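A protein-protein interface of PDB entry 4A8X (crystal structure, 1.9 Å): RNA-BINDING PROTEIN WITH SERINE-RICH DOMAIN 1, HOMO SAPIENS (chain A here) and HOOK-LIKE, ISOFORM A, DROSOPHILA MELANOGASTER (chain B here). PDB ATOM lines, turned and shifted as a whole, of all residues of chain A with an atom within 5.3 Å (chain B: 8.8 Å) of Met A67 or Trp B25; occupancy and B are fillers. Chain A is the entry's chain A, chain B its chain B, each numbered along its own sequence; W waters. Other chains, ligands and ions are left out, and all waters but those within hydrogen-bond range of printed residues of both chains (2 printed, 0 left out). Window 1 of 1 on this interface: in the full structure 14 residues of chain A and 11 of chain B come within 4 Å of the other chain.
OG1 of Thr A27 touches CH2 of Trp B25 (3.6 Å).
CZ3 of Trp B25 touches OH of Tyr A28 (3.7 Å).
Leu B28 touches Lys A65.
Pro B27 touches His A66 (CA to O, 3.4 Å).
Trp B25 touches Met A67 (CE3 to CE, 3.8 Å).
Pro B27 touches Met A67 (CA to SD, 3.6 Å).
Leu B26 touches Gly A70.
CB of Trp B25 touches O of Gln A71, 3.2 Å away.
Ile B23 touches Ile A72 (CD1 to CG2, 3.7 Å).
Ile A72 touches Tyr B24.
Of the printed residues of chain B, Thr A27 touches Trp B25.
Ala A63 touches none of the printed residues of chain B.
Met A67 touches two residues of chain B.
Printed residues of chain B within 4 Å of Asp A68: Leu B28.
Gly A70 touches one residue of chain B.
Trp B25 touches just these residues of chain A: Ile A24 (3.7 Å), Thr A27 (3.6 Å), Tyr A28 (3.7 Å), Met A67 (3.8 Å) and Gln A71 (3.2 Å).
Thr B29 touches none of the printed residues of chain A.
The nearest residue of chain B that does not touch Met A67 is Leu B26 (4.2 Å).
The nearest printed residue of chain A that does not touch Leu B26 is Met A67 (4.2 Å).
The backbone carbonyl oxygen of Lys A62 is in hydrogen-bond range of a ring nitrogen (ND1) of His A66 (2.9 Å).
The backbone carbonyl oxygen (O) of Arg B15 lies within hydrogen-bond range of the backbone NH (N) of Trp B25 (2.8 Å).
The side-chain carboxylate of Asp A68 is in hydrogen-bond range of the backbone NH of Ala A79, 2.8 Å away.
The backbone carbonyl oxygen of Ile A24 is in hydrogen-bond range of the side-chain hydroxyl of Thr A27.
The backbone NH (N) of Gly A69 sits at hydrogen-bond distance from the backbone carbonyl oxygen (O) of Ile A77 (3.0 Å).
O of Gly A70 lies within hydrogen-bond range of N of Ile A77 (2.9 Å).
The backbone carbonyl oxygen (O) of Tyr B24 sits at hydrogen-bond distance from the backbone NH (N) of Asp A73 (2.8 Å).
The backbone carbonyl oxygen of Leu B26 is in hydrogen-bond range of the backbone NH of Gln A71 (2.8 Å).
O of His A66 sits at hydrogen-bond distance from N of Leu B28 (2.9 Å).
Of the 19 printed residues of chain A, 12 touch a printed residue of chain B.
Hydrophobic or aromatic side chains of chain A within 4 Å of the printed part of chain B: Ile A24, Tyr A28, His A66, Met A67 and Ile A72.
Along chain A the printed residues that touch a printed residue of chain B span positions 24 to 73.
Hydrophobic or aromatic side chains of chain B within 4 Å of the printed part of chain A: Ile B23, Trp B25, Leu B26, Pro B27, Leu B28 and Ile B33.
Water W1 bridges OD1 of Asp A73 (2.5 Å) and N of Tyr B24 (2.9 Å).
Water W2 lies within hydrogen-bond range of O of Leu B26 (2.8 Å), NE2 of Gln A71 (2.8 Å) and O of Pro B27 (3.3 Å).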
ATOM      1  N   ILE A  24      17.136  23.221  16.410  1.00  0.00           N
ATOM      2  CA  ILE A  24      16.041  23.428  15.496  1.00  0.00           C
ATOM      3  C   ILE A  24      14.870  22.456  15.799  1.00  0.00           C
ATOM      4  O   ILE A  24      13.715  22.861  15.862  1.00  0.00           O
ATOM      5  CB  ILE A  24      16.542  23.256  14.022  1.00  0.00           C
ATOM      6  CG1 ILE A  24      17.392  24.471  13.614  1.00  0.00           C
ATOM      7  CG2 ILE A  24      15.390  23.052  13.084  1.00  0.00           C
ATOM      8  CD1 ILE A  24      18.206  24.237  12.311  1.00  0.00           C
ATOM      9  N   PHE A  25      15.165  21.182  15.957  1.00  0.00           N
ATOM     10  CA  PHE A  25      14.109  20.182  16.046  1.00  0.00           C
ATOM     11  C   PHE A  25      13.498  20.083  17.449  1.00  0.00           C
ATOM     12  O   PHE A  25      12.381  19.578  17.639  1.00  0.00           O
ATOM     13  CB  PHE A  25      14.633  18.861  15.497  1.00  0.00           C
ATOM     14  CG  PHE A  25      14.609  18.849  13.994  1.00  0.00           C
ATOM     15  CD1 PHE A  25      13.469  18.487  13.330  1.00  0.00           C
ATOM     16  CD2 PHE A  25      15.701  19.305  13.259  1.00  0.00           C
ATOM     17  CE1 PHE A  25      13.407  18.543  11.922  1.00  0.00           C
ATOM     18  CE2 PHE A  25      15.643  19.370  11.863  1.00  0.00           C
ATOM     19  CZ  PHE A  25      14.475  18.979  11.205  1.00  0.00           C
ATOM     20  N   THR A  27      12.393  22.533  18.774  1.00  0.00           N
ATOM     21  CA  THR A  27      11.180  23.325  18.530  1.00  0.00           C
ATOM     22  C   THR A  27       9.919  22.437  18.544  1.00  0.00           C
ATOM     23  O   THR A  27       8.838  22.919  18.877  1.00  0.00           O
ATOM     24  CB  THR A  27      11.230  24.087  17.141  1.00  0.00           C
ATOM     25  OG1 THR A  27      12.398  24.907  17.077  1.00  0.00           O
ATOM     26  CG2 THR A  27      10.001  25.012  16.953  1.00  0.00           C
ATOM     27  N   TYR A  28      10.052  21.169  18.144  1.00  0.00           N
ATOM     28  CA  TYR A  28       8.877  20.340  17.861  1.00  0.00           C
ATOM     29  C   TYR A  28       8.619  19.277  18.941  1.00  0.00           C
ATOM     30  O   TYR A  28       7.609  18.578  18.883  1.00  0.00           O
ATOM     31  CB  TYR A  28       8.937  19.725  16.428  1.00  0.00           C
ATOM     32  CG  TYR A  28       9.087  20.819  15.415  1.00  0.00           C
ATOM     33  CD1 TYR A  28       8.035  21.654  15.124  1.00  0.00           C
ATOM     34  CD2 TYR A  28      10.316  21.070  14.783  1.00  0.00           C
ATOM     35  CE1 TYR A  28       8.154  22.705  14.233  1.00  0.00           C
ATOM     36  CE2 TYR A  28      10.451  22.145  13.898  1.00  0.00           C
ATOM     37  CZ  TYR A  28       9.365  22.941  13.613  1.00  0.00           C
ATOM     38  OH  TYR A  28       9.464  24.001  12.743  1.00  0.00           O
ATOM     39  N   LYS A  62       4.658  16.231  14.229  1.00  0.00           N
ATOM     40  CA  LYS A  62       4.732  17.696  14.176  1.00  0.00           C
ATOM     41  C   LYS A  62       5.975  18.149  13.430  1.00  0.00           C
ATOM     42  O   LYS A  62       5.924  19.092  12.611  1.00  0.00           O
ATOM     43  CB  LYS A  62       4.770  18.301  15.571  1.00  0.00           C
ATOM     44  CG  LYS A  62       4.440  19.810  15.587  1.00  0.00           C
ATOM     45  CD  LYS A  62       4.453  20.392  16.999  1.00  0.00           C
ATOM     46  CE  LYS A  62       4.386  21.929  16.966  1.00  0.00           C
ATOM     47  NZ  LYS A  62       4.268  22.534  18.339  1.00  0.00           N
ATOM     48  N   ALA A  63       7.084  17.499  13.739  1.00  0.00           N
ATOM     49  CA  ALA A  63       8.346  17.830  13.065  1.00  0.00           C
ATOM     50  C   ALA A  63       8.245  17.570  11.575  1.00  0.00           C
ATOM     51  O   ALA A  63       8.686  18.384  10.752  1.00  0.00           O
ATOM     52  CB  ALA A  63       9.495  17.039  13.638  1.00  0.00           C
ATOM     53  N   LEU A  64       7.684  16.429  11.219  1.00  0.00           N
ATOM     54  CA  LEU A  64       7.523  16.079   9.805  1.00  0.00           C
ATOM     55  C   LEU A  64       6.603  17.085   9.095  1.00  0.00           C
ATOM     56  O   LEU A  64       6.883  17.517   7.987  1.00  0.00           O
ATOM     57  CB  LEU A  64       6.928  14.674   9.683  1.00  0.00           C
ATOM     58  CG  LEU A  64       7.801  13.500  10.162  1.00  0.00           C
ATOM     59  CD1 LEU A  64       7.018  12.194  10.162  1.00  0.00           C
ATOM     60  CD2 LEU A  64       9.037  13.343   9.262  1.00  0.00           C
ATOM     61  N   LYS A  65       5.489  17.395   9.749  1.00  0.00           N
ATOM     62  CA  LYS A  65       4.524  18.404   9.307  1.00  0.00           C
ATOM     63  C   LYS A  65       5.177  19.778   8.958  1.00  0.00           C
ATOM     64  O   LYS A  65       4.948  20.314   7.860  1.00  0.00           O
ATOM     65  CB  LYS A  65       3.459  18.531  10.419  1.00  0.00           C
ATOM     66  CG  LYS A  65       2.234  19.329  10.091  1.00  0.00           C
ATOM     67  CD  LYS A  65       1.202  19.298  11.247  1.00  0.00           C
ATOM     68  CE  LYS A  65       0.305  20.538  11.199  1.00  0.00           C
ATOM     69  NZ  LYS A  65      -0.653  20.646  12.335  1.00  0.00           N
ATOM     70  N   HIS A  66       6.004  20.316   9.865  1.00  0.00           N
ATOM     71  CA  HIS A  66       6.634  21.633   9.691  1.00  0.00           C
ATOM     72  C   HIS A  66       7.948  21.646   8.911  1.00  0.00           C
ATOM     73  O   HIS A  66       8.345  22.692   8.406  1.00  0.00           O
ATOM     74  CB  HIS A  66       6.860  22.301  11.054  1.00  0.00           C
ATOM     75  CG  HIS A  66       5.583  22.619  11.771  1.00  0.00           C
ATOM     76  ND1 HIS A  66       4.716  21.642  12.203  1.00  0.00           N
ATOM     77  CD2 HIS A  66       5.008  23.802  12.084  1.00  0.00           C
ATOM     78  CE1 HIS A  66       3.661  22.209  12.771  1.00  0.00           C
ATOM     79  NE2 HIS A  66       3.817  23.516  12.713  1.00  0.00           N
ATOM     80  N   MET A  67       8.648  20.524   8.818  1.00  0.00           N
ATOM     81  CA  MET A  67      10.013  20.583   8.280  1.00  0.00           C
ATOM     82  C   MET A  67      10.331  19.696   7.063  1.00  0.00           C
ATOM     83  O   MET A  67      11.404  19.827   6.487  1.00  0.00           O
ATOM     84  CB  MET A  67      11.026  20.313   9.394  1.00  0.00           C
ATOM     85  CG  MET A  67      11.213  21.498  10.338  1.00  0.00           C
ATOM     86  SD  MET A  67      11.784  23.057   9.572  1.00  0.00           S
ATOM     87  CE  MET A  67      13.572  22.769   9.458  1.00  0.00           C
ATOM     88  N   ASP A  68       9.420  18.824   6.643  1.00  0.00           N
ATOM     89  CA  ASP A  68       9.649  18.086   5.421  1.00  0.00           C
ATOM     90  C   ASP A  68       9.371  19.082   4.303  1.00  0.00           C
ATOM     91  O   ASP A  68       8.235  19.498   4.126  1.00  0.00           O
ATOM     92  CB  ASP A  68       8.744  16.883   5.277  1.00  0.00           C
ATOM     93  CG  ASP A  68       8.994  16.154   3.988  1.00  0.00           C
ATOM     94  OD1 ASP A  68      10.171  15.965   3.594  1.00  0.00           O
ATOM     95  OD2 ASP A  68       8.019  15.763   3.351  1.00  0.00           O
ATOM     96  N   GLY A  69      10.411  19.540   3.614  1.00  0.00           N
ATOM     97  CA  GLY A  69      10.242  20.673   2.714  1.00  0.00           C
ATOM     98  C   GLY A  69      10.572  22.022   3.308  1.00  0.00           C
ATOM     99  O   GLY A  69      10.482  23.045   2.615  1.00  0.00           O
ATOM    100  N   GLY A  70      10.962  22.037   4.589  1.00  0.00           N
ATOM    101  CA  GLY A  70      11.396  23.246   5.268  1.00  0.00           C
ATOM    102  C   GLY A  70      12.828  23.551   4.795  1.00  0.00           C
ATOM    103  O   GLY A  70      13.353  22.883   3.874  1.00  0.00           O
ATOM    104  N   GLN A  71      13.425  24.569   5.377  1.00  0.00           N
ATOM    105  CA  GLN A  71      14.763  25.018   4.976  1.00  0.00           C
ATOM    106  C   GLN A  71      15.714  25.097   6.145  1.00  0.00           C
ATOM    107  O   GLN A  71      15.335  25.558   7.211  1.00  0.00           O
ATOM    108  CB  GLN A  71      14.692  26.411   4.335  1.00  0.00           C
ATOM    109  CG  GLN A  71      13.893  26.456   3.046  1.00  0.00           C
ATOM    110  CD  GLN A  71      13.659  27.880   2.598  1.00  0.00           C
ATOM    111  OE1 GLN A  71      14.576  28.540   2.122  1.00  0.00           O
ATOM    112  NE2 GLN A  71      12.433  28.380   2.781  1.00  0.00           N
ATOM    113  N   ILE A  72      16.963  24.671   5.927  1.00  0.00           N
ATOM    114  CA  ILE A  72      18.036  24.825   6.905  1.00  0.00           C
ATOM    115  C   ILE A  72      19.317  25.276   6.175  1.00  0.00           C
ATOM    116  O   ILE A  72      19.725  24.654   5.181  1.00  0.00           O
ATOM    117  CB  ILE A  72      18.305  23.531   7.707  1.00  0.00           C
ATOM    118  CG1 ILE A  72      17.039  22.995   8.433  1.00  0.00           C
ATOM    119  CG2 ILE A  72      19.481  23.785   8.719  1.00  0.00           C
ATOM    120  CD1 ILE A  72      17.269  21.724   9.327  1.00  0.00           C
ATOM    121  N   ASP A  73      19.904  26.355   6.665  1.00  0.00           N
ATOM    122  CA  ASP A  73      21.053  27.022   6.045  1.00  0.00           C
ATOM    123  C   ASP A  73      20.906  27.224   4.547  1.00  0.00           C
ATOM    124  O   ASP A  73      21.820  26.874   3.775  1.00  0.00           O
ATOM    125  CB  ASP A  73      22.352  26.242   6.326  1.00  0.00           C
ATOM    126  CG  ASP A  73      23.584  27.007   5.916  1.00  0.00           C
ATOM    127  OD1 ASP A  73      23.582  28.261   5.990  1.00  0.00           O
ATOM    128  OD2 ASP A  73      24.569  26.336   5.504  1.00  0.00           O
ATOM    129  N   ILE A  77      15.198  20.909   2.911  1.00  0.00           N
ATOM    130  CA  ILE A  77      15.553  19.607   3.522  1.00  0.00           C
ATOM    131  C   ILE A  77      14.377  18.633   3.383  1.00  0.00           C
ATOM    132  O   ILE A  77      13.266  19.033   3.054  1.00  0.00           O
ATOM    133  CB  ILE A  77      15.879  19.712   5.046  1.00  0.00           C
ATOM    134  CG1 ILE A  77      14.652  20.213   5.809  1.00  0.00           C
ATOM    135  CG2 ILE A  77      17.097  20.639   5.324  1.00  0.00           C
ATOM    136  CD1 ILE A  77      14.643  19.779   7.261  1.00  0.00           C
ATOM    137  N   THR A  78      14.652  17.359   3.579  1.00  0.00           N
ATOM    138  CA  THR A  78      13.615  16.314   3.599  1.00  0.00           C
ATOM    139  C   THR A  78      13.468  15.824   5.052  1.00  0.00           C
ATOM    140  O   THR A  78      14.428  15.855   5.813  1.00  0.00           O
ATOM    141  CB  THR A  78      13.991  15.117   2.718  1.00  0.00           C
ATOM    142  OG1 THR A  78      15.231  14.526   3.168  1.00  0.00           O
ATOM    143  CG2 THR A  78      14.125  15.547   1.247  1.00  0.00           C
ATOM    144  N   ALA A  79      12.270  15.412   5.428  1.00  0.00           N
ATOM    145  CA  ALA A  79      12.031  14.840   6.752  1.00  0.00           C
ATOM    146  C   ALA A  79      11.082  13.661   6.584  1.00  0.00           C
ATOM    147  O   ALA A  79      10.011  13.797   5.982  1.00  0.00           O
ATOM    148  CB  ALA A  79      11.457  15.881   7.703  1.00  0.00           C
ATOM    149  N   LEU B  10      16.430  40.329   7.722  1.00  0.00           N
ATOM    150  CA  LEU B  10      16.606  38.865   7.729  1.00  0.00           C
ATOM    151  C   LEU B  10      15.977  38.228   8.967  1.00  0.00           C
ATOM    152  O   LEU B  10      15.339  37.174   8.882  1.00  0.00           O
ATOM    153  CB  LEU B  10      18.070  38.438   7.674  1.00  0.00           C
ATOM    154  CG  LEU B  10      18.865  38.676   6.396  1.00  0.00           C
ATOM    155  CD1 LEU B  10      20.213  37.959   6.521  1.00  0.00           C
ATOM    156  CD2 LEU B  10      18.091  38.205   5.172  1.00  0.00           C
ATOM    157  N   ASP B  11      16.156  38.871  10.114  1.00  0.00           N
ATOM    158  CA  ASP B  11      15.679  38.319  11.375  1.00  0.00           C
ATOM    159  C   ASP B  11      14.151  38.398  11.525  1.00  0.00           C
ATOM    160  O   ASP B  11      13.567  37.661  12.310  1.00  0.00           O
ATOM    161  CB  ASP B  11      16.420  38.989  12.532  1.00  0.00           C
ATOM    162  CG  ASP B  11      17.919  38.709  12.480  1.00  0.00           C
ATOM    163  OD1 ASP B  11      18.314  37.566  12.814  1.00  0.00           O
ATOM    164  OD2 ASP B  11      18.694  39.608  12.061  1.00  0.00           O
ATOM    165  N   LEU B  13      12.309  37.760   8.816  1.00  0.00           N
ATOM    166  CA  LEU B  13      11.848  36.809   7.810  1.00  0.00           C
ATOM    167  C   LEU B  13      12.157  35.365   8.165  1.00  0.00           C
ATOM    168  O   LEU B  13      11.333  34.483   7.949  1.00  0.00           O
ATOM    169  CB  LEU B  13      12.473  37.149   6.446  1.00  0.00           C
ATOM    170  CG  LEU B  13      12.104  38.530   5.893  1.00  0.00           C
ATOM    171  CD1 LEU B  13      12.735  38.749   4.531  1.00  0.00           C
ATOM    172  CD2 LEU B  13      10.609  38.663   5.802  1.00  0.00           C
ATOM    173  N   PHE B  14      13.331  35.140   8.753  1.00  0.00           N
ATOM    174  CA  PHE B  14      13.900  33.822   8.921  1.00  0.00           C
ATOM    175  C   PHE B  14      14.335  33.606  10.365  1.00  0.00           C
ATOM    176  O   PHE B  14      14.591  34.568  11.066  1.00  0.00           O
ATOM    177  CB  PHE B  14      15.138  33.680   8.000  1.00  0.00           C
ATOM    178  CG  PHE B  14      14.841  34.041   6.571  1.00  0.00           C
ATOM    179  CD1 PHE B  14      13.948  33.284   5.836  1.00  0.00           C
ATOM    180  CD2 PHE B  14      15.417  35.143   5.986  1.00  0.00           C
ATOM    181  CE1 PHE B  14      13.646  33.609   4.539  1.00  0.00           C
ATOM    182  CE2 PHE B  14      15.129  35.460   4.676  1.00  0.00           C
ATOM    183  CZ  PHE B  14      14.242  34.702   3.957  1.00  0.00           C
ATOM    184  N   ARG B  15      14.443  32.343  10.778  1.00  0.00           N
ATOM    185  CA  ARG B  15      14.891  31.990  12.119  1.00  0.00           C
ATOM    186  C   ARG B  15      16.386  31.836  12.122  1.00  0.00           C
ATOM    187  O   ARG B  15      16.951  31.397  11.152  1.00  0.00           O
ATOM    188  CB  ARG B  15      14.217  30.690  12.552  1.00  0.00           C
ATOM    189  CG  ARG B  15      12.669  30.859  12.541  1.00  0.00           C
ATOM    190  CD  ARG B  15      11.934  29.740  13.217  1.00  0.00           C
ATOM    191  NE  ARG B  15      10.488  29.917  13.048  1.00  0.00           N
ATOM    192  CZ  ARG B  15       9.573  29.190  13.678  1.00  0.00           C
ATOM    193  NH1 ARG B  15       9.960  28.228  14.515  1.00  0.00           N
ATOM    194  NH2 ARG B  15       8.273  29.417  13.473  1.00  0.00           N
ATOM    195  N   LYS B  16      17.038  32.199  13.210  1.00  0.00           N
ATOM    196  CA  LYS B  16      18.493  32.098  13.250  1.00  0.00           C
ATOM    197  C   LYS B  16      18.896  31.271  14.463  1.00  0.00           C
ATOM    198  O   LYS B  16      18.353  31.469  15.556  1.00  0.00           O
ATOM    199  CB  LYS B  16      19.096  33.497  13.307  1.00  0.00           C
ATOM    200  CG  LYS B  16      20.581  33.548  13.173  1.00  0.00           C
ATOM    201  CD  LYS B  16      21.082  34.982  13.317  1.00  0.00           C
ATOM    202  CE  LYS B  16      22.581  35.073  12.942  1.00  0.00           C
ATOM    203  NZ  LYS B  16      23.223  36.416  13.122  1.00  0.00           N
ATOM    204  N   THR B  17      19.853  30.361  14.290  1.00  0.00           N
ATOM    205  CA  THR B  17      20.342  29.569  15.410  1.00  0.00           C
ATOM    206  C   THR B  17      21.225  30.410  16.357  1.00  0.00           C
ATOM    207  O   THR B  17      21.878  31.381  15.954  1.00  0.00           O
ATOM    208  CB  THR B  17      21.136  28.310  14.930  1.00  0.00           C
ATOM    209  OG1 THR B  17      22.351  28.701  14.279  1.00  0.00           O
ATOM    210  CG2 THR B  17      20.317  27.495  13.903  1.00  0.00           C
ATOM    211  N   LYS B  18      21.241  30.008  17.616  1.00  0.00           N
ATOM    212  CA  LYS B  18      22.208  30.514  18.565  1.00  0.00           C
ATOM    213  C   LYS B  18      23.478  29.702  18.398  1.00  0.00           C
ATOM    214  O   LYS B  18      24.576  30.225  18.543  1.00  0.00           O
ATOM    215  CB  LYS B  18      21.669  30.397  19.995  1.00  0.00           C
ATOM    216  CG  LYS B  18      20.485  31.306  20.287  1.00  0.00           C
ATOM    217  N   GLY B  19      23.357  28.417  18.086  1.00  0.00           N
ATOM    218  CA  GLY B  19      24.556  27.599  17.913  1.00  0.00           C
ATOM    219  C   GLY B  19      25.429  28.091  16.752  1.00  0.00           C
ATOM    220  O   GLY B  19      24.899  28.488  15.704  1.00  0.00           O
ATOM    221  N   CYS B  22      26.437  30.698  13.118  1.00  0.00           N
ATOM    222  CA  CYS B  22      24.991  30.870  13.092  1.00  0.00           C
ATOM    223  C   CYS B  22      24.460  30.661  11.673  1.00  0.00           C
ATOM    224  O   CYS B  22      25.027  31.176  10.708  1.00  0.00           O
ATOM    225  CB  CYS B  22      24.595  32.249  13.608  1.00  0.00           C
ATOM    226  SG  CYS B  22      25.171  32.568  15.262  1.00  0.00           S
ATOM    227  N   ILE B  23      23.373  29.898  11.568  1.00  0.00           N
ATOM    228  CA  ILE B  23      22.714  29.660  10.304  1.00  0.00           C
ATOM    229  C   ILE B  23      21.264  30.052  10.438  1.00  0.00           C
ATOM    230  O   ILE B  23      20.716  30.094  11.541  1.00  0.00           O
ATOM    231  CB  ILE B  23      22.779  28.176   9.847  1.00  0.00           C
ATOM    232  CG1 ILE B  23      22.173  27.222  10.897  1.00  0.00           C
ATOM    233  CG2 ILE B  23      24.174  27.818   9.551  1.00  0.00           C
ATOM    234  CD1 ILE B  23      22.046  25.771  10.453  1.00  0.00           C
ATOM    235  N   TYR B  24      20.645  30.344   9.306  1.00  0.00           N
ATOM    236  CA  TYR B  24      19.222  30.632   9.289  1.00  0.00           C
ATOM    237  C   TYR B  24      18.453  29.371   8.917  1.00  0.00           C
ATOM    238  O   TYR B  24      18.999  28.444   8.285  1.00  0.00           O
ATOM    239  CB  TYR B  24      18.898  31.755   8.327  1.00  0.00           C
ATOM    240  CG  TYR B  24      19.341  33.119   8.805  1.00  0.00           C
ATOM    241  CD1 TYR B  24      18.503  33.919   9.556  1.00  0.00           C
ATOM    242  CD2 TYR B  24      20.615  33.600   8.513  1.00  0.00           C
ATOM    243  CE1 TYR B  24      18.909  35.168  10.012  1.00  0.00           C
ATOM    244  CE2 TYR B  24      21.044  34.827   8.978  1.00  0.00           C
ATOM    245  CZ  TYR B  24      20.177  35.624   9.704  1.00  0.00           C
ATOM    246  OH  TYR B  24      20.603  36.841  10.141  1.00  0.00           O
ATOM    247  N   TRP B  25      17.186  29.334   9.303  1.00  0.00           N
ATOM    248  CA  TRP B  25      16.295  28.231   8.925  1.00  0.00           C
ATOM    249  C   TRP B  25      14.846  28.684   8.908  1.00  0.00           C
ATOM    250  O   TRP B  25      14.517  29.769   9.402  1.00  0.00           O
ATOM    251  CB  TRP B  25      16.438  27.044   9.880  1.00  0.00           C
ATOM    252  CG  TRP B  25      16.017  27.264  11.307  1.00  0.00           C
ATOM    253  CD1 TRP B  25      16.711  27.900  12.259  1.00  0.00           C
ATOM    254  CD2 TRP B  25      14.818  26.768  11.934  1.00  0.00           C
ATOM    255  NE1 TRP B  25      16.024  27.865  13.466  1.00  0.00           N
ATOM    256  CE2 TRP B  25      14.856  27.169  13.285  1.00  0.00           C
ATOM    257  CE3 TRP B  25      13.722  26.022  11.479  1.00  0.00           C
ATOM    258  CZ2 TRP B  25      13.841  26.850  14.193  1.00  0.00           C
ATOM    259  CZ3 TRP B  25      12.705  25.704  12.380  1.00  0.00           C
ATOM    260  CH2 TRP B  25      12.774  26.130  13.723  1.00  0.00           C
ATOM    261  N   LEU B  26      13.975  27.865   8.326  1.00  0.00           N
ATOM    262  CA  LEU B  26      12.604  28.280   8.175  1.00  0.00           C
ATOM    263  C   LEU B  26      11.707  27.088   7.918  1.00  0.00           C
ATOM    264  O   LEU B  26      11.912  26.340   6.961  1.00  0.00           O
ATOM    265  CB  LEU B  26      12.484  29.274   7.012  1.00  0.00           C
ATOM    266  CG  LEU B  26      11.112  29.894   6.853  1.00  0.00           C
ATOM    267  CD1 LEU B  26      10.868  30.865   7.985  1.00  0.00           C
ATOM    268  CD2 LEU B  26      10.941  30.553   5.478  1.00  0.00           C
ATOM    269  N   PRO B  27      10.717  26.894   8.787  1.00  0.00           N
ATOM    270  CA  PRO B  27       9.724  25.844   8.574  1.00  0.00           C
ATOM    271  C   PRO B  27       8.710  26.220   7.502  1.00  0.00           C
ATOM    272  O   PRO B  27       8.675  27.338   6.980  1.00  0.00           O
ATOM    273  CB  PRO B  27       9.041  25.724   9.941  1.00  0.00           C
ATOM    274  CG  PRO B  27       9.154  27.099  10.527  1.00  0.00           C
ATOM    275  CD  PRO B  27      10.510  27.607  10.066  1.00  0.00           C
ATOM    276  N   LEU B  28       7.903  25.258   7.119  1.00  0.00           N
ATOM    277  CA  LEU B  28       6.839  25.546   6.163  1.00  0.00           C
ATOM    278  C   LEU B  28       5.879  26.538   6.775  1.00  0.00           C
ATOM    279  O   LEU B  28       5.682  26.558   8.004  1.00  0.00           O
ATOM    280  CB  LEU B  28       6.087  24.274   5.812  1.00  0.00           C
ATOM    281  CG  LEU B  28       6.877  23.255   4.999  1.00  0.00           C
ATOM    282  CD1 LEU B  28       6.023  21.990   4.809  1.00  0.00           C
ATOM    283  CD2 LEU B  28       7.282  23.908   3.674  1.00  0.00           C
ATOM    284  N   THR B  29       5.300  27.377   5.919  1.00  0.00           N
ATOM    285  CA  THR B  29       4.267  28.307   6.343  1.00  0.00           C
ATOM    286  C   THR B  29       3.012  27.530   6.743  1.00  0.00           C
ATOM    287  O   THR B  29       2.703  26.461   6.158  1.00  0.00           O
ATOM    288  CB  THR B  29       3.908  29.312   5.205  1.00  0.00           C
ATOM    289  OG1 THR B  29       3.529  28.590   4.030  1.00  0.00           O
ATOM    290  CG2 THR B  29       5.107  30.186   4.857  1.00  0.00           C
ATOM    291  N   ILE B  33       1.543  23.953   5.113  1.00  0.00           N
ATOM    292  CA  ILE B  33       1.196  22.720   5.816  1.00  0.00           C
ATOM    293  C   ILE B  33      -0.243  22.270   5.499  1.00  0.00           C
ATOM    294  O   ILE B  33      -0.505  21.097   5.182  1.00  0.00           O
ATOM    295  CB  ILE B  33       1.328  22.913   7.321  1.00  0.00           C
ATOM    296  CG1 ILE B  33       2.778  23.259   7.685  1.00  0.00           C
ATOM    297  CG2 ILE B  33       0.893  21.657   8.050  1.00  0.00           C
ATOM    298  CD1 ILE B  33       2.930  23.807   9.101  1.00  0.00           C
HETATM  299  O   HOH W   1      22.131  30.167   6.824  1.00  0.00           O
HETATM  300  O   HOH W   2      10.796  26.965   4.522  1.00  0.00           O
